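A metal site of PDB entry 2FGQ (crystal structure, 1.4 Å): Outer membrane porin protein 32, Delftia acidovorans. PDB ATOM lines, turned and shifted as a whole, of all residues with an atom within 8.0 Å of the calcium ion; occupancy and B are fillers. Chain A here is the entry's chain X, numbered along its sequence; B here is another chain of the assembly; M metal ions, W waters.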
ATOM      1  N   ASN A  13     -26.120  -8.095  18.574  1.00  0.00           N
ATOM      2  CA  ASN A  13     -26.542  -9.414  19.048  1.00  0.00           C
ATOM      3  C   ASN A  13     -26.781  -9.427  20.549  1.00  0.00           C
ATOM      4  O   ASN A  13     -26.406  -8.527  21.284  1.00  0.00           O
ATOM      5  CB  ASN A  13     -25.513 -10.527  18.657  1.00  0.00           C
ATOM      6  CG  ASN A  13     -24.092 -10.200  19.102  1.00  0.00           C
ATOM      7  OD1 ASN A  13     -23.833  -9.994  20.310  1.00  0.00           O
ATOM      8  ND2 ASN A  13     -23.135 -10.179  18.158  1.00  0.00           N
ATOM      9  N   TYR A  27     -23.496 -12.363  30.165  1.00  0.00           N
ATOM     10  CA  TYR A  27     -24.344 -12.211  29.017  1.00  0.00           C
ATOM     11  C   TYR A  27     -24.674 -10.758  28.807  1.00  0.00           C
ATOM     12  O   TYR A  27     -24.518  -9.923  29.695  1.00  0.00           O
ATOM     13  CB  TYR A  27     -25.563 -13.072  29.166  1.00  0.00           C
ATOM     14  CG  TYR A  27     -26.376 -12.686  30.348  1.00  0.00           C
ATOM     15  CD1 TYR A  27     -27.375 -11.770  30.229  1.00  0.00           C
ATOM     16  CD2 TYR A  27     -26.108 -13.230  31.607  1.00  0.00           C
ATOM     17  CE1 TYR A  27     -28.139 -11.393  31.318  1.00  0.00           C
ATOM     18  CE2 TYR A  27     -26.854 -12.811  32.734  1.00  0.00           C
ATOM     19  CZ  TYR A  27     -27.862 -11.889  32.561  1.00  0.00           C
ATOM     20  OH  TYR A  27     -28.654 -11.464  33.635  1.00  0.00           O
ATOM     21  N   GLY A  28     -25.094 -10.445  27.601  1.00  0.00           N
ATOM     22  CA  GLY A  28     -25.203  -9.029  27.267  1.00  0.00           C
ATOM     23  C   GLY A  28     -25.602  -8.755  25.853  1.00  0.00           C
ATOM     24  O   GLY A  28     -25.967  -9.662  25.099  1.00  0.00           O
ATOM     25  N   LEU A  29     -25.503  -7.474  25.495  1.00  0.00           N
ATOM     26  CA  LEU A  29     -25.758  -7.015  24.139  1.00  0.00           C
ATOM     27  C   LEU A  29     -24.370  -6.789  23.545  1.00  0.00           C
ATOM     28  O   LEU A  29     -23.621  -5.978  24.075  1.00  0.00           O
ATOM     29  CB  LEU A  29     -26.599  -5.742  24.102  1.00  0.00           C
ATOM     30  CG  LEU A  29     -27.185  -5.448  22.704  1.00  0.00           C
ATOM     31  CD1 LEU A  29     -28.392  -6.344  22.460  1.00  0.00           C
ATOM     32  CD2 LEU A  29     -27.500  -3.994  22.533  1.00  0.00           C
ATOM     33  N   GLY A  30     -24.037  -7.468  22.485  1.00  0.00           N
ATOM     34  CA  GLY A  30     -22.767  -7.324  21.808  1.00  0.00           C
ATOM     35  C   GLY A  30     -22.943  -6.992  20.346  1.00  0.00           C
ATOM     36  O   GLY A  30     -24.003  -6.621  19.879  1.00  0.00           O
ATOM     37  N   THR A  31     -21.839  -7.080  19.611  1.00  0.00           N
ATOM     38  CA  THR A  31     -21.821  -6.672  18.216  1.00  0.00           C
ATOM     39  C   THR A  31     -21.058  -7.610  17.326  1.00  0.00           C
ATOM     40  O   THR A  31     -20.229  -8.415  17.804  1.00  0.00           O
ATOM     41  CB  THR A  31     -21.222  -5.242  18.062  1.00  0.00           C
ATOM     42  OG1 THR A  31     -19.832  -5.226  18.488  1.00  0.00           O
ATOM     43  CG2 THR A  31     -21.995  -4.203  18.892  1.00  0.00           C
ATOM     44  N   GLY A  63     -22.624  -0.765  18.144  1.00  0.00           N
ATOM     45  CA  GLY A  63     -24.003  -0.364  18.356  1.00  0.00           C
ATOM     46  C   GLY A  63     -24.440  -0.494  19.791  1.00  0.00           C
ATOM     47  O   GLY A  63     -25.343   0.212  20.209  1.00  0.00           O
ATOM     48  N   ASP A  64     -23.796  -1.328  20.581  1.00  0.00           N
ATOM     49  CA  ASP A  64     -24.200  -1.475  21.981  1.00  0.00           C
ATOM     50  C   ASP A  64     -23.850  -0.277  22.868  1.00  0.00           C
ATOM     51  O   ASP A  64     -24.524  -0.070  23.876  1.00  0.00           O
ATOM     52  CB  ASP A  64     -23.674  -2.788  22.597  1.00  0.00           C
ATOM     53  CG  ASP A  64     -22.154  -2.917  22.569  1.00  0.00           C
ATOM     54  OD1 ASP A  64     -21.433  -2.282  21.741  1.00  0.00           O
ATOM     55  OD2 ASP A  64     -21.621  -3.648  23.450  1.00  0.00           O
ATOM     56  N   ASP A  65     -22.861   0.513  22.483  1.00  0.00           N
ATOM     57  CA  ASP A  65     -22.467   1.687  23.244  1.00  0.00           C
ATOM     58  C   ASP A  65     -22.310   2.967  22.462  1.00  0.00           C
ATOM     59  O   ASP A  65     -21.797   3.950  22.991  1.00  0.00           O
ATOM     60  CB  ASP A  65     -21.281   1.401  24.161  1.00  0.00           C
ATOM     61  CG  ASP A  65     -19.961   1.341  23.440  1.00  0.00           C
ATOM     62  OD1 ASP A  65     -19.837   1.693  22.236  1.00  0.00           O
ATOM     63  OD2 ASP A  65     -18.945   1.000  24.070  1.00  0.00           O
ATOM     64  N   ALA A 307     -16.739 -12.843  22.285  1.00  0.00           N
ATOM     65  CA  ALA A 307     -18.110 -12.305  22.236  1.00  0.00           C
ATOM     66  C   ALA A 307     -17.999 -10.781  22.362  1.00  0.00           C
ATOM     67  O   ALA A 307     -18.085 -10.246  23.479  1.00  0.00           O
ATOM     68  CB  ALA A 307     -19.004 -12.871  23.350  1.00  0.00           C
ATOM     69  N   LYS A 308     -17.733 -10.098  21.250  1.00  0.00           N
ATOM     70  CA  LYS A 308     -17.425  -8.667  21.253  1.00  0.00           C
ATOM     71  C   LYS A 308     -18.591  -7.908  21.872  1.00  0.00           C
ATOM     72  O   LYS A 308     -19.745  -8.121  21.484  1.00  0.00           O
ATOM     73  CB  LYS A 308     -17.176  -8.163  19.854  1.00  0.00           C
ATOM     74  CG  LYS A 308     -16.778  -6.708  19.787  1.00  0.00           C
ATOM     75  CD  LYS A 308     -16.380  -6.301  18.345  1.00  0.00           C
ATOM     76  CE  LYS A 308     -14.912  -6.564  18.044  1.00  0.00           C
ATOM     77  NZ  LYS A 308     -14.545  -6.258  16.641  1.00  0.00           N
ATOM     78  N   GLY A 309     -18.259  -7.027  22.802  1.00  0.00           N
ATOM     79  CA  GLY A 309     -19.233  -6.208  23.513  1.00  0.00           C
ATOM     80  C   GLY A 309     -19.843  -6.908  24.696  1.00  0.00           C
ATOM     81  O   GLY A 309     -20.668  -6.300  25.382  1.00  0.00           O
ATOM     82  N   VAL A 310     -19.469  -8.157  24.936  1.00  0.00           N
ATOM     83  CA  VAL A 310     -19.984  -8.879  26.103  1.00  0.00           C
ATOM     84  C   VAL A 310     -18.833  -9.387  26.959  1.00  0.00           C
ATOM     85  O   VAL A 310     -18.658  -8.955  28.090  1.00  0.00           O
ATOM     86  CB  VAL A 310     -20.999  -9.994  25.732  1.00  0.00           C
ATOM     87  CG1 VAL A 310     -21.449 -10.765  26.986  1.00  0.00           C
ATOM     88  CG2 VAL A 310     -22.195  -9.368  25.056  1.00  0.00           C
ATOM     89  N   TYR A 311     -18.041 -10.303  26.399  1.00  0.00           N
ATOM     90  CA  TYR A 311     -16.846 -10.768  27.085  1.00  0.00           C
ATOM     91  C   TYR A 311     -15.932 -11.388  26.028  1.00  0.00           C
ATOM     92  O   TYR A 311     -16.350 -12.286  25.286  1.00  0.00           O
ATOM     93  CB  TYR A 311     -17.173 -11.796  28.172  1.00  0.00           C
ATOM     94  CG  TYR A 311     -15.925 -12.176  28.958  1.00  0.00           C
ATOM     95  CD1 TYR A 311     -15.315 -11.279  29.814  1.00  0.00           C
ATOM     96  CD2 TYR A 311     -15.286 -13.415  28.735  1.00  0.00           C
ATOM     97  CE1 TYR A 311     -14.131 -11.596  30.466  1.00  0.00           C
ATOM     98  CE2 TYR A 311     -14.080 -13.746  29.409  1.00  0.00           C
ATOM     99  CZ  TYR A 311     -13.518 -12.834  30.260  1.00  0.00           C
ATOM    100  OH  TYR A 311     -12.351 -13.111  30.938  1.00  0.00           O
ATOM    101  N   ASN B 135     -26.613   2.038  27.504  1.00  0.00           N
ATOM    102  CA  ASN B 135     -25.894   1.023  26.712  1.00  0.00           C
ATOM    103  C   ASN B 135     -26.600  -0.309  26.798  1.00  0.00           C
ATOM    104  O   ASN B 135     -27.329  -0.602  27.757  1.00  0.00           O
ATOM    105  CB  ASN B 135     -24.466   0.844  27.258  1.00  0.00           C
ATOM    106  CG  ASN B 135     -23.593   2.115  27.191  1.00  0.00           C
ATOM    107  OD1 ASN B 135     -22.694   2.355  28.037  1.00  0.00           O
ATOM    108  ND2 ASN B 135     -23.811   2.880  26.223  1.00  0.00           N
ATOM    109  N   ASN B 136     -26.357  -1.132  25.790  1.00  0.00           N
ATOM    110  CA  ASN B 136     -26.746  -2.558  25.853  1.00  0.00           C
ATOM    111  C   ASN B 136     -28.235  -2.727  26.001  1.00  0.00           C
ATOM    112  O   ASN B 136     -28.709  -3.687  26.624  1.00  0.00           O
ATOM    113  CB  ASN B 136     -26.071  -3.233  27.039  1.00  0.00           C
ATOM    114  CG  ASN B 136     -24.541  -2.978  27.049  1.00  0.00           C
ATOM    115  OD1 ASN B 136     -23.879  -3.070  26.006  1.00  0.00           O
ATOM    116  ND2 ASN B 136     -23.998  -2.605  28.209  1.00  0.00           N
ATOM    117  N   LEU B 137     -28.985  -1.851  25.331  1.00  0.00           N
ATOM    118  CA  LEU B 137     -30.436  -1.748  25.456  1.00  0.00           C
ATOM    119  C   LEU B 137     -31.216  -2.534  24.358  1.00  0.00           C
ATOM    120  O   LEU B 137     -30.871  -2.505  23.172  1.00  0.00           O
ATOM    121  CB  LEU B 137     -30.799  -0.260  25.401  1.00  0.00           C
ATOM    122  CG  LEU B 137     -32.290   0.072  25.493  1.00  0.00           C
ATOM    123  CD1 LEU B 137     -32.872  -0.244  26.870  1.00  0.00           C
ATOM    124  CD2 LEU B 137     -32.458   1.531  25.176  1.00  0.00           C
ATOM    125  N   PHE B 156     -28.731  -4.642  29.578  1.00  0.00           N
ATOM    126  CA  PHE B 156     -27.851  -5.546  30.268  1.00  0.00           C
ATOM    127  C   PHE B 156     -26.704  -4.820  31.000  1.00  0.00           C
ATOM    128  O   PHE B 156     -26.055  -3.945  30.460  1.00  0.00           O
ATOM    129  CB  PHE B 156     -27.215  -6.515  29.269  1.00  0.00           C
ATOM    130  CG  PHE B 156     -28.196  -7.381  28.529  1.00  0.00           C
ATOM    131  CD1 PHE B 156     -28.719  -6.981  27.324  1.00  0.00           C
ATOM    132  CD2 PHE B 156     -28.547  -8.624  29.020  1.00  0.00           C
ATOM    133  CE1 PHE B 156     -29.601  -7.796  26.640  1.00  0.00           C
ATOM    134  CE2 PHE B 156     -29.448  -9.454  28.337  1.00  0.00           C
ATOM    135  CZ  PHE B 156     -29.987  -9.034  27.155  1.00  0.00           C
ATOM    136  N   ASP B 157     -26.430  -5.245  32.212  1.00  0.00           N
ATOM    137  CA  ASP B 157     -25.305  -4.749  32.982  1.00  0.00           C
ATOM    138  C   ASP B 157     -23.980  -5.333  32.580  1.00  0.00           C
ATOM    139  O   ASP B 157     -22.958  -4.652  32.707  1.00  0.00           O
ATOM    140  CB  ASP B 157     -25.527  -5.003  34.472  1.00  0.00           C
ATOM    141  CG  ASP B 157     -25.881  -6.415  34.765  1.00  0.00           C
ATOM    142  OD1 ASP B 157     -24.990  -7.254  35.091  1.00  0.00           O
ATOM    143  OD2 ASP B 157     -27.068  -6.798  34.642  1.00  0.00           O
ATOM    144  N   GLU B 158     -24.010  -6.558  32.103  1.00  0.00           N
ATOM    145  CA  GLU B 158     -22.786  -7.244  31.654  1.00  0.00           C
ATOM    146  C   GLU B 158     -21.732  -7.362  32.763  1.00  0.00           C
ATOM    147  O   GLU B 158     -20.517  -7.354  32.523  1.00  0.00           O
ATOM    148  CB  GLU B 158     -22.195  -6.561  30.398  1.00  0.00           C
ATOM    149  CG  GLU B 158     -23.246  -6.514  29.320  1.00  0.00           C
ATOM    150  CD  GLU B 158     -22.877  -5.818  28.032  1.00  0.00           C
ATOM    151  OE1 GLU B 158     -21.837  -5.120  27.969  1.00  0.00           O
ATOM    152  OE2 GLU B 158     -23.708  -5.947  27.087  1.00  0.00           O
HETATM  153 CA    CA M   1     -22.254  -4.676  25.520  1.00  0.00          CA
HETATM  154  O   HOH W   1     -20.561  -3.017  26.202  1.00  0.00           O
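Five residues have an atom within 4 Å of the calcium ion: Leu 29, Asp 64, Gly 309, Asn 136 of chain B and Glu 158 of chain B. The nearest printed residue that does not touch the calcium ion is Gly 30 (4.5 Å).
The calcium ion is bound by O of Gly 309 (2.3 Å), OD1 of Asn 136 of chain B (2.3 Å), O of Leu 29 (2.4 Å), OD2 of Asp 64 (2.4 Å), water W1 (2.5 Å), OE2 of Glu 158 of chain B (2.5 Å) and OE1 of Glu 158 of chain B (2.5 Å).
O of Asn 136 of chain B is in hydrogen-bond range of N of Phe 156 of chain B (3.1 Å).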
